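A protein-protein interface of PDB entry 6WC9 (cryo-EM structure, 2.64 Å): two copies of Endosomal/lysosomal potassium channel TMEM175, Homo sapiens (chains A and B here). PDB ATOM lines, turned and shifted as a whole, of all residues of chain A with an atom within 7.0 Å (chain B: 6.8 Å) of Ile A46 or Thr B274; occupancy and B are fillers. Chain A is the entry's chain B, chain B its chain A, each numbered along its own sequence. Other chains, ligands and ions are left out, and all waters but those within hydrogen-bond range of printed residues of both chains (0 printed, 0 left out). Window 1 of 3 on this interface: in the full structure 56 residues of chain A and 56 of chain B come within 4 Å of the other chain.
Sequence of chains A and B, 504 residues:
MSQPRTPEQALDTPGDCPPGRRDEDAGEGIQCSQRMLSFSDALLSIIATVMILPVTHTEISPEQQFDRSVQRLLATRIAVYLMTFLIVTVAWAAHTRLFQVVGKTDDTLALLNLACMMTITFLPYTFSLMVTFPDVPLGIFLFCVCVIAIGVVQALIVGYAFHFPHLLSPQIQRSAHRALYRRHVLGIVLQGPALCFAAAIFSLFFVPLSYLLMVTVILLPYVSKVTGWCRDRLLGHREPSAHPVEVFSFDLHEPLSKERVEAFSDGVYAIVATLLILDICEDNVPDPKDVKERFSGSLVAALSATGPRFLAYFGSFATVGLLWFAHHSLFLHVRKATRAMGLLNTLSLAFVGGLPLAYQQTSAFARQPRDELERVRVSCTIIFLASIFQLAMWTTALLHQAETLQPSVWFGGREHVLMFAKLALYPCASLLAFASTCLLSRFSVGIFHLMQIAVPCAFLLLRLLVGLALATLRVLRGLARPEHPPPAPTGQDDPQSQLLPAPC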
ATOM      1  N   SER A  40      18.792  24.389 -24.696  1.00  0.00           N
ATOM      2  CA  SER A  40      18.755  25.276 -23.540  1.00  0.00           C
ATOM      3  C   SER A  40      17.697  26.361 -23.706  1.00  0.00           C
ATOM      4  O   SER A  40      16.968  26.676 -22.758  1.00  0.00           O
ATOM      5  CB  SER A  40      20.134  25.895 -23.323  1.00  0.00           C
ATOM      6  OG  SER A  40      21.136  24.902 -23.301  1.00  0.00           O
ATOM      7  N   ASP A  41      17.608  26.952 -24.899  1.00  0.00           N
ATOM      8  CA  ASP A  41      16.600  27.976 -25.150  1.00  0.00           C
ATOM      9  C   ASP A  41      15.195  27.418 -24.984  1.00  0.00           C
ATOM     10  O   ASP A  41      14.322  28.078 -24.413  1.00  0.00           O
ATOM     11  CB  ASP A  41      16.773  28.551 -26.553  1.00  0.00           C
ATOM     12  CG  ASP A  41      17.789  29.668 -26.607  1.00  0.00           C
ATOM     13  OD1 ASP A  41      17.888  30.440 -25.632  1.00  0.00           O
ATOM     14  OD2 ASP A  41      18.495  29.773 -27.631  1.00  0.00           O
ATOM     15  N   ALA A  42      14.954  26.211 -25.493  1.00  0.00           N
ATOM     16  CA  ALA A  42      13.643  25.589 -25.336  1.00  0.00           C
ATOM     17  C   ALA A  42      13.304  25.384 -23.864  1.00  0.00           C
ATOM     18  O   ALA A  42      12.206  25.734 -23.408  1.00  0.00           O
ATOM     19  CB  ALA A  42      13.609  24.263 -26.089  1.00  0.00           C
ATOM     20  N   LEU A  43      14.237  24.807 -23.104  1.00  0.00           N
ATOM     21  CA  LEU A  43      13.996  24.603 -21.679  1.00  0.00           C
ATOM     22  C   LEU A  43      13.711  25.921 -20.973  1.00  0.00           C
ATOM     23  O   LEU A  43      12.778  26.015 -20.167  1.00  0.00           O
ATOM     24  CB  LEU A  43      15.193  23.904 -21.038  1.00  0.00           C
ATOM     25  CG  LEU A  43      15.343  22.407 -21.292  1.00  0.00           C
ATOM     26  CD1 LEU A  43      16.707  21.948 -20.855  1.00  0.00           C
ATOM     27  CD2 LEU A  43      14.269  21.624 -20.570  1.00  0.00           C
ATOM     28  N   LEU A  44      14.506  26.952 -21.262  1.00  0.00           N
ATOM     29  CA  LEU A  44      14.350  28.224 -20.569  1.00  0.00           C
ATOM     30  C   LEU A  44      13.041  28.901 -20.945  1.00  0.00           C
ATOM     31  O   LEU A  44      12.406  29.547 -20.105  1.00  0.00           O
ATOM     32  CB  LEU A  44      15.540  29.127 -20.881  1.00  0.00           C
ATOM     33  CG  LEU A  44      16.799  28.840 -20.063  1.00  0.00           C
ATOM     34  CD1 LEU A  44      18.042  29.325 -20.785  1.00  0.00           C
ATOM     35  CD2 LEU A  44      16.696  29.461 -18.689  1.00  0.00           C
ATOM     36  N   SER A  45      12.619  28.765 -22.201  1.00  0.00           N
ATOM     37  CA  SER A  45      11.331  29.306 -22.611  1.00  0.00           C
ATOM     38  C   SER A  45      10.188  28.603 -21.896  1.00  0.00           C
ATOM     39  O   SER A  45       9.206  29.246 -21.508  1.00  0.00           O
ATOM     40  CB  SER A  45      11.177  29.190 -24.125  1.00  0.00           C
ATOM     41  OG  SER A  45      11.258  27.845 -24.554  1.00  0.00           O
ATOM     42  N   ILE A  46      10.289  27.286 -21.715  1.00  0.00           N
ATOM     43  CA  ILE A  46       9.265  26.581 -20.950  1.00  0.00           C
ATOM     44  C   ILE A  46       9.250  27.067 -19.507  1.00  0.00           C
ATOM     45  O   ILE A  46       8.186  27.306 -18.926  1.00  0.00           O
ATOM     46  CB  ILE A  46       9.485  25.061 -21.027  1.00  0.00           C
ATOM     47  CG1 ILE A  46       9.221  24.566 -22.442  1.00  0.00           C
ATOM     48  CG2 ILE A  46       8.583  24.344 -20.046  1.00  0.00           C
ATOM     49  CD1 ILE A  46       9.732  23.196 -22.706  1.00  0.00           C
ATOM     50  N   ILE A  47      10.431  27.221 -18.906  1.00  0.00           N
ATOM     51  CA  ILE A  47      10.513  27.596 -17.501  1.00  0.00           C
ATOM     52  C   ILE A  47      10.070  29.031 -17.260  1.00  0.00           C
ATOM     53  O   ILE A  47       9.608  29.353 -16.161  1.00  0.00           O
ATOM     54  CB  ILE A  47      11.948  27.375 -16.986  1.00  0.00           C
ATOM     55  CG1 ILE A  47      12.309  25.889 -17.023  1.00  0.00           C
ATOM     56  CG2 ILE A  47      12.114  27.922 -15.583  1.00  0.00           C
ATOM     57  CD1 ILE A  47      11.344  24.987 -16.293  1.00  0.00           C
ATOM     58  N   ALA A  48      10.196  29.908 -18.254  1.00  0.00           N
ATOM     59  CA  ALA A  48       9.802  31.299 -18.069  1.00  0.00           C
ATOM     60  C   ALA A  48       8.292  31.492 -18.148  1.00  0.00           C
ATOM     61  O   ALA A  48       7.771  32.463 -17.591  1.00  0.00           O
ATOM     62  CB  ALA A  48      10.497  32.178 -19.105  1.00  0.00           C
ATOM     63  N   THR A  49       7.580  30.592 -18.825  1.00  0.00           N
ATOM     64  CA  THR A  49       6.135  30.675 -18.978  1.00  0.00           C
ATOM     65  C   THR A  49       5.390  29.722 -18.049  1.00  0.00           C
ATOM     66  O   THR A  49       4.216  29.427 -18.290  1.00  0.00           O
ATOM     67  CB  THR A  49       5.737  30.388 -20.426  1.00  0.00           C
ATOM     68  OG1 THR A  49       6.020  29.020 -20.737  1.00  0.00           O
ATOM     69  CG2 THR A  49       6.487  31.283 -21.386  1.00  0.00           C
ATOM     70  N   VAL A  50       6.043  29.238 -16.995  1.00  0.00           N
ATOM     71  CA  VAL A  50       5.410  28.242 -16.138  1.00  0.00           C
ATOM     72  C   VAL A  50       4.371  28.875 -15.222  1.00  0.00           C
ATOM     73  O   VAL A  50       3.390  28.223 -14.850  1.00  0.00           O
ATOM     74  CB  VAL A  50       6.474  27.478 -15.329  1.00  0.00           C
ATOM     75  CG1 VAL A  50       7.229  28.411 -14.405  1.00  0.00           C
ATOM     76  CG2 VAL A  50       5.832  26.358 -14.529  1.00  0.00           C
ATOM     77  N   MET A  51       4.553  30.137 -14.845  1.00  0.00           N
ATOM     78  CA  MET A  51       3.658  30.801 -13.910  1.00  0.00           C
ATOM     79  C   MET A  51       2.472  31.468 -14.592  1.00  0.00           C
ATOM     80  O   MET A  51       1.694  32.152 -13.922  1.00  0.00           O
ATOM     81  CB  MET A  51       4.429  31.831 -13.088  1.00  0.00           C
ATOM     82  CG  MET A  51       5.100  31.250 -11.862  1.00  0.00           C
ATOM     83  SD  MET A  51       3.923  30.671 -10.633  1.00  0.00           S
ATOM     84  CE  MET A  51       4.598  29.055 -10.302  1.00  0.00           C
ATOM     85  N   LEU A  53       0.265  29.519 -16.249  1.00  0.00           N
ATOM     86  CA  LEU A  53      -0.810  28.532 -16.171  1.00  0.00           C
ATOM     87  C   LEU A  53      -1.717  28.787 -14.976  1.00  0.00           C
ATOM     88  O   LEU A  53      -2.948  28.712 -15.133  1.00  0.00           O
ATOM     89  CB  LEU A  53      -0.213  27.125 -16.146  1.00  0.00           C
ATOM     90  CG  LEU A  53       0.328  26.651 -17.493  1.00  0.00           C
ATOM     91  CD1 LEU A  53       1.668  25.974 -17.318  1.00  0.00           C
ATOM     92  CD2 LEU A  53      -0.656  25.724 -18.174  1.00  0.00           C
ATOM     93  N   VAL A  88      13.939  34.575 -14.929  1.00  0.00           N
ATOM     94  CA  VAL A  88      14.408  33.531 -15.830  1.00  0.00           C
ATOM     95  C   VAL A  88      15.035  34.143 -17.073  1.00  0.00           C
ATOM     96  O   VAL A  88      15.961  33.568 -17.652  1.00  0.00           O
ATOM     97  CB  VAL A  88      13.262  32.570 -16.195  1.00  0.00           C
ATOM     98  CG1 VAL A  88      13.749  31.512 -17.165  1.00  0.00           C
ATOM     99  CG2 VAL A  88      12.706  31.916 -14.955  1.00  0.00           C
ATOM    100  N   THR A 121      15.633  25.561 -13.408  1.00  0.00           N
ATOM    101  CA  THR A 121      14.251  25.095 -13.346  1.00  0.00           C
ATOM    102  C   THR A 121      13.618  25.296 -11.975  1.00  0.00           C
ATOM    103  O   THR A 121      12.389  25.232 -11.862  1.00  0.00           O
ATOM    104  CB  THR A 121      14.182  23.621 -13.726  1.00  0.00           C
ATOM    105  OG1 THR A 121      15.030  22.859 -12.859  1.00  0.00           O
ATOM    106  CG2 THR A 121      14.617  23.423 -15.161  1.00  0.00           C
ATOM    107  N   PHE A 264      14.479  31.717 -28.165  1.00  0.00           N
ATOM    108  CA  PHE A 264      13.713  31.984 -26.953  1.00  0.00           C
ATOM    109  C   PHE A 264      12.344  32.569 -27.283  1.00  0.00           C
ATOM    110  O   PHE A 264      11.315  32.128 -26.748  1.00  0.00           O
ATOM    111  CB  PHE A 264      14.533  32.925 -26.070  1.00  0.00           C
ATOM    112  CG  PHE A 264      13.973  33.138 -24.703  1.00  0.00           C
ATOM    113  CD1 PHE A 264      14.111  32.176 -23.728  1.00  0.00           C
ATOM    114  CD2 PHE A 264      13.335  34.318 -24.384  1.00  0.00           C
ATOM    115  CE1 PHE A 264      13.604  32.379 -22.472  1.00  0.00           C
ATOM    116  CE2 PHE A 264      12.827  34.521 -23.131  1.00  0.00           C
ATOM    117  CZ  PHE A 264      12.963  33.551 -22.173  1.00  0.00           C
ATOM    118  N   GLY A 267       9.995  29.956 -28.836  1.00  0.00           N
ATOM    119  CA  GLY A 267       9.438  29.074 -27.827  1.00  0.00           C
ATOM    120  C   GLY A 267       8.319  29.724 -27.038  1.00  0.00           C
ATOM    121  O   GLY A 267       7.257  29.126 -26.825  1.00  0.00           O
ATOM    122  N   VAL A 268       8.548  30.955 -26.578  1.00  0.00           N
ATOM    123  CA  VAL A 268       7.512  31.667 -25.834  1.00  0.00           C
ATOM    124  C   VAL A 268       6.248  31.791 -26.678  1.00  0.00           C
ATOM    125  O   VAL A 268       5.132  31.539 -26.204  1.00  0.00           O
ATOM    126  CB  VAL A 268       8.026  33.046 -25.380  1.00  0.00           C
ATOM    127  CG1 VAL A 268       6.921  33.836 -24.704  1.00  0.00           C
ATOM    128  CG2 VAL A 268       9.203  32.894 -24.446  1.00  0.00           C
ATOM    129  N   ILE A 271       4.365  28.393 -27.026  1.00  0.00           N
ATOM    130  CA  ILE A 271       3.683  28.033 -25.786  1.00  0.00           C
ATOM    131  C   ILE A 271       2.425  28.873 -25.605  1.00  0.00           C
ATOM    132  O   ILE A 271       1.351  28.356 -25.264  1.00  0.00           O
ATOM    133  CB  ILE A 271       4.640  28.186 -24.590  1.00  0.00           C
ATOM    134  CG1 ILE A 271       5.765  27.162 -24.690  1.00  0.00           C
ATOM    135  CG2 ILE A 271       3.891  28.036 -23.280  1.00  0.00           C
ATOM    136  CD1 ILE A 271       6.937  27.459 -23.806  1.00  0.00           C
ATOM    137  N   GLY B 267      12.487  19.547 -28.854  1.00  0.00           N
ATOM    138  CA  GLY B 267      11.256  19.999 -28.229  1.00  0.00           C
ATOM    139  C   GLY B 267      10.597  18.920 -27.394  1.00  0.00           C
ATOM    140  O   GLY B 267      10.179  19.162 -26.254  1.00  0.00           O
ATOM    141  N   TYR B 269      11.990  16.343 -26.013  1.00  0.00           N
ATOM    142  CA  TYR B 269      12.819  16.070 -24.845  1.00  0.00           C
ATOM    143  C   TYR B 269      12.635  17.134 -23.772  1.00  0.00           C
ATOM    144  O   TYR B 269      12.511  16.813 -22.585  1.00  0.00           O
ATOM    145  CB  TYR B 269      14.287  15.978 -25.260  1.00  0.00           C
ATOM    146  CG  TYR B 269      14.730  14.608 -25.721  1.00  0.00           C
ATOM    147  CD1 TYR B 269      14.624  13.510 -24.891  1.00  0.00           C
ATOM    148  CD2 TYR B 269      15.270  14.419 -26.981  1.00  0.00           C
ATOM    149  CE1 TYR B 269      15.027  12.266 -25.301  1.00  0.00           C
ATOM    150  CE2 TYR B 269      15.676  13.177 -27.400  1.00  0.00           C
ATOM    151  CZ  TYR B 269      15.553  12.102 -26.557  1.00  0.00           C
ATOM    152  OH  TYR B 269      15.956  10.857 -26.966  1.00  0.00           O
ATOM    153  N   ALA B 270      12.620  18.407 -24.168  1.00  0.00           N
ATOM    154  CA  ALA B 270      12.440  19.482 -23.199  1.00  0.00           C
ATOM    155  C   ALA B 270      11.091  19.374 -22.496  1.00  0.00           C
ATOM    156  O   ALA B 270      11.003  19.487 -21.264  1.00  0.00           O
ATOM    157  CB  ALA B 270      12.580  20.832 -23.897  1.00  0.00           C
ATOM    158  N   ILE B 271      10.024  19.161 -23.267  1.00  0.00           N
ATOM    159  CA  ILE B 271       8.696  19.036 -22.672  1.00  0.00           C
ATOM    160  C   ILE B 271       8.665  17.886 -21.674  1.00  0.00           C
ATOM    161  O   ILE B 271       8.143  18.018 -20.557  1.00  0.00           O
ATOM    162  CB  ILE B 271       7.636  18.858 -23.771  1.00  0.00           C
ATOM    163  CG1 ILE B 271       7.535  20.129 -24.608  1.00  0.00           C
ATOM    164  CG2 ILE B 271       6.290  18.503 -23.169  1.00  0.00           C
ATOM    165  CD1 ILE B 271       6.823  19.943 -25.913  1.00  0.00           C
ATOM    166  N   VAL B 272       9.210  16.734 -22.067  1.00  0.00           N
ATOM    167  CA  VAL B 272       9.134  15.559 -21.207  1.00  0.00           C
ATOM    168  C   VAL B 272       9.996  15.733 -19.966  1.00  0.00           C
ATOM    169  O   VAL B 272       9.671  15.201 -18.899  1.00  0.00           O
ATOM    170  CB  VAL B 272       9.525  14.302 -22.001  1.00  0.00           C
ATOM    171  CG1 VAL B 272       9.577  13.098 -21.095  1.00  0.00           C
ATOM    172  CG2 VAL B 272       8.546  14.073 -23.133  1.00  0.00           C
ATOM    173  N   ALA B 273      11.096  16.477 -20.072  1.00  0.00           N
ATOM    174  CA  ALA B 273      11.939  16.733 -18.915  1.00  0.00           C
ATOM    175  C   ALA B 273      11.352  17.766 -17.965  1.00  0.00           C
ATOM    176  O   ALA B 273      11.713  17.770 -16.784  1.00  0.00           O
ATOM    177  CB  ALA B 273      13.321  17.193 -19.368  1.00  0.00           C
ATOM    178  N   THR B 274      10.467  18.640 -18.442  1.00  0.00           N
ATOM    179  CA  THR B 274       9.931  19.710 -17.608  1.00  0.00           C
ATOM    180  C   THR B 274       8.493  19.485 -17.150  1.00  0.00           C
ATOM    181  O   THR B 274       7.969  20.304 -16.384  1.00  0.00           O
ATOM    182  CB  THR B 274      10.022  21.039 -18.353  1.00  0.00           C
ATOM    183  OG1 THR B 274       9.604  20.858 -19.709  1.00  0.00           O
ATOM    184  CG2 THR B 274      11.443  21.557 -18.327  1.00  0.00           C
ATOM    185  N   LEU B 275       7.831  18.426 -17.620  1.00  0.00           N
ATOM    186  CA  LEU B 275       6.448  18.174 -17.217  1.00  0.00           C
ATOM    187  C   LEU B 275       6.272  18.214 -15.701  1.00  0.00           C
ATOM    188  O   LEU B 275       5.383  18.900 -15.176  1.00  0.00           O
ATOM    189  CB  LEU B 275       5.999  16.818 -17.756  1.00  0.00           C
ATOM    190  CG  LEU B 275       5.401  16.772 -19.158  1.00  0.00           C
ATOM    191  CD1 LEU B 275       5.451  15.351 -19.674  1.00  0.00           C
ATOM    192  CD2 LEU B 275       3.984  17.300 -19.162  1.00  0.00           C
ATOM    193  N   LEU B 276       7.100  17.457 -14.980  1.00  0.00           N
ATOM    194  CA  LEU B 276       6.875  17.273 -13.551  1.00  0.00           C
ATOM    195  C   LEU B 276       7.150  18.550 -12.772  1.00  0.00           C
ATOM    196  O   LEU B 276       6.438  18.859 -11.813  1.00  0.00           O
ATOM    197  CB  LEU B 276       7.738  16.126 -13.033  1.00  0.00           C
ATOM    198  CG  LEU B 276       7.464  14.743 -13.631  1.00  0.00           C
ATOM    199  CD1 LEU B 276       8.209  13.688 -12.861  1.00  0.00           C
ATOM    200  CD2 LEU B 276       5.987  14.415 -13.658  1.00  0.00           C
ATOM    201  N   ILE B 277       8.172  19.310 -13.164  1.00  0.00           N
ATOM    202  CA  ILE B 277       8.434  20.574 -12.484  1.00  0.00           C
ATOM    203  C   ILE B 277       7.321  21.570 -12.770  1.00  0.00           C
ATOM    204  O   ILE B 277       6.951  22.371 -11.903  1.00  0.00           O
ATOM    205  CB  ILE B 277       9.815  21.127 -12.878  1.00  0.00           C
ATOM    206  CG1 ILE B 277      10.195  22.314 -11.997  1.00  0.00           C
ATOM    207  CG2 ILE B 277       9.856  21.521 -14.336  1.00  0.00           C
ATOM    208  CD1 ILE B 277      10.367  21.966 -10.555  1.00  0.00           C
ATOM    209  N   LEU B 278       6.762  21.541 -13.982  1.00  0.00           N
ATOM    210  CA  LEU B 278       5.605  22.381 -14.266  1.00  0.00           C
ATOM    211  C   LEU B 278       4.458  22.055 -13.320  1.00  0.00           C
ATOM    212  O   LEU B 278       3.866  22.951 -12.701  1.00  0.00           O
ATOM    213  CB  LEU B 278       5.171  22.193 -15.717  1.00  0.00           C
ATOM    214  CG  LEU B 278       5.641  23.240 -16.722  1.00  0.00           C
ATOM    215  CD1 LEU B 278       7.147  23.440 -16.663  1.00  0.00           C
ATOM    216  CD2 LEU B 278       5.213  22.818 -18.098  1.00  0.00           C
ATOM    217  N   ASP B 279       4.134  20.768 -13.192  1.00  0.00           N
ATOM    218  CA  ASP B 279       3.036  20.376 -12.313  1.00  0.00           C
ATOM    219  C   ASP B 279       3.328  20.740 -10.861  1.00  0.00           C
ATOM    220  O   ASP B 279       2.428  21.167 -10.127  1.00  0.00           O
ATOM    221  CB  ASP B 279       2.763  18.882 -12.450  1.00  0.00           C
ATOM    222  CG  ASP B 279       1.789  18.572 -13.565  1.00  0.00           C
ATOM    223  OD1 ASP B 279       2.236  18.381 -14.716  1.00  0.00           O
ATOM    224  OD2 ASP B 279       0.571  18.531 -13.293  1.00  0.00           O
ATOM    225  N   TYR B 313      10.934  14.273 -10.167  1.00  0.00           N
ATOM    226  CA  TYR B 313      11.370  15.255 -11.151  1.00  0.00           C
ATOM    227  C   TYR B 313      12.869  15.162 -11.390  1.00  0.00           C
ATOM    228  O   TYR B 313      13.326  15.228 -12.535  1.00  0.00           O
ATOM    229  CB  TYR B 313      10.989  16.663 -10.697  1.00  0.00           C
ATOM    230  CG  TYR B 313      11.742  17.752 -11.420  1.00  0.00           C
ATOM    231  CD1 TYR B 313      11.683  17.862 -12.800  1.00  0.00           C
ATOM    232  CD2 TYR B 313      12.517  18.664 -10.724  1.00  0.00           C
ATOM    233  CE1 TYR B 313      12.373  18.842 -13.464  1.00  0.00           C
ATOM    234  CE2 TYR B 313      13.205  19.653 -11.382  1.00  0.00           C
ATOM    235  CZ  TYR B 313      13.130  19.739 -12.751  1.00  0.00           C
ATOM    236  OH  TYR B 313      13.820  20.727 -13.406  1.00  0.00           O
ATOM    237  N   SER B 316      13.550  11.971 -13.489  1.00  0.00           N
ATOM    238  CA  SER B 316      13.062  12.115 -14.854  1.00  0.00           C
ATOM    239  C   SER B 316      13.928  13.081 -15.646  1.00  0.00           C
ATOM    240  O   SER B 316      14.272  12.811 -16.802  1.00  0.00           O
ATOM    241  CB  SER B 316      11.610  12.584 -14.838  1.00  0.00           C
ATOM    242  OG  SER B 316      11.097  12.704 -16.150  1.00  0.00           O
ATOM    243  N   PHE B 317      14.289  14.216 -15.047  1.00  0.00           N
ATOM    244  CA  PHE B 317      15.124  15.182 -15.744  1.00  0.00           C
ATOM    245  C   PHE B 317      16.478  14.582 -16.081  1.00  0.00           C
ATOM    246  O   PHE B 317      16.964  14.723 -17.205  1.00  0.00           O
ATOM    247  CB  PHE B 317      15.284  16.443 -14.898  1.00  0.00           C
ATOM    248  CG  PHE B 317      15.929  17.580 -15.628  1.00  0.00           C
ATOM    249  CD1 PHE B 317      15.162  18.546 -16.246  1.00  0.00           C
ATOM    250  CD2 PHE B 317      17.304  17.681 -15.702  1.00  0.00           C
ATOM    251  CE1 PHE B 317      15.751  19.584 -16.916  1.00  0.00           C
ATOM    252  CE2 PHE B 317      17.894  18.719 -16.373  1.00  0.00           C
ATOM    253  CZ  PHE B 317      17.118  19.671 -16.981  1.00  0.00           C
ATOM    254  N   VAL B 320      15.989  11.879 -18.944  1.00  0.00           N
ATOM    255  CA  VAL B 320      15.655  12.478 -20.230  1.00  0.00           C
ATOM    256  C   VAL B 320      16.831  13.281 -20.767  1.00  0.00           C
ATOM    257  O   VAL B 320      17.092  13.291 -21.974  1.00  0.00           O
ATOM    258  CB  VAL B 320      14.390  13.346 -20.098  1.00  0.00           C
ATOM    259  CG1 VAL B 320      14.083  14.017 -21.407  1.00  0.00           C
ATOM    260  CG2 VAL B 320      13.213  12.506 -19.664  1.00  0.00           C
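Printed residues of chain A within 4 Å of Thr B274: Leu A43 (3.6 Å), Ile A46 (3.6 Å) and Ile A47 (3.99 Å).
Printed residues of chain A within 4 Å of Tyr B313: Thr A121 (2.5 Å).
Of the printed residues of chain B, Leu A43 touches Ala B270 and Thr B274.
Of the printed residues of chain A, Leu B278 touches Ile A46 and Val A50.
Printed residues of chain A within 4 Å of Ile B277: Thr A121 (3.7 Å).
Val B320 touches none of the printed residues of chain A.
Ala A42 touches none of the printed residues of chain B.
The nearest residue of chain B that does not touch Ile A46 is Ile B271 (4.1 Å).
The nearest printed residue of chain A that does not touch Thr B274 is Thr A121 (4.9 Å).
OH of Tyr B313 is in hydrogen-bond range of OG1 of Thr A121 (2.5 Å).
Hydrophobic or aromatic side chains of chain B that line the printed part of chain A: Ala B270, Ile B277, Leu B278 and Tyr B313.
Among the printed residues, no Asp or Glu carboxylate lies within 4 Å of a Lys or Arg side-chain nitrogen of the other chain.
The backbone carbonyl oxygen of Ile A46 is in hydrogen-bond range of the side-chain hydroxyl of Thr A49, 3.3 Å away.
The backbone carbonyl oxygen (O) of Ile B271 lies within hydrogen-bond range of the side-chain hydroxyl (OG1) of Thr B274 (3.3 Å).
The backbone carbonyl oxygen (O) of Ala B270 is in hydrogen-bond range of the side-chain hydroxyl (OG1) of Thr B274 (2.5 Å).
CD2 of Leu A43 touches CB of Ala B270, 3.8 Å away.
CG2 of Thr B274 touches CD2 of Leu A43, at 3.6 Å.
Ile A46 touches Ala B270.
Thr B274 touches Ile A46.
Ile A46 touches Leu B278.
Thr B274 touches Ile A47 (CG2 to CD1, 3.99 Å).
Leu B278 touches Val A50.
Ile B277 touches Thr A121.
Positions printed for both chains: 267 and 271.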
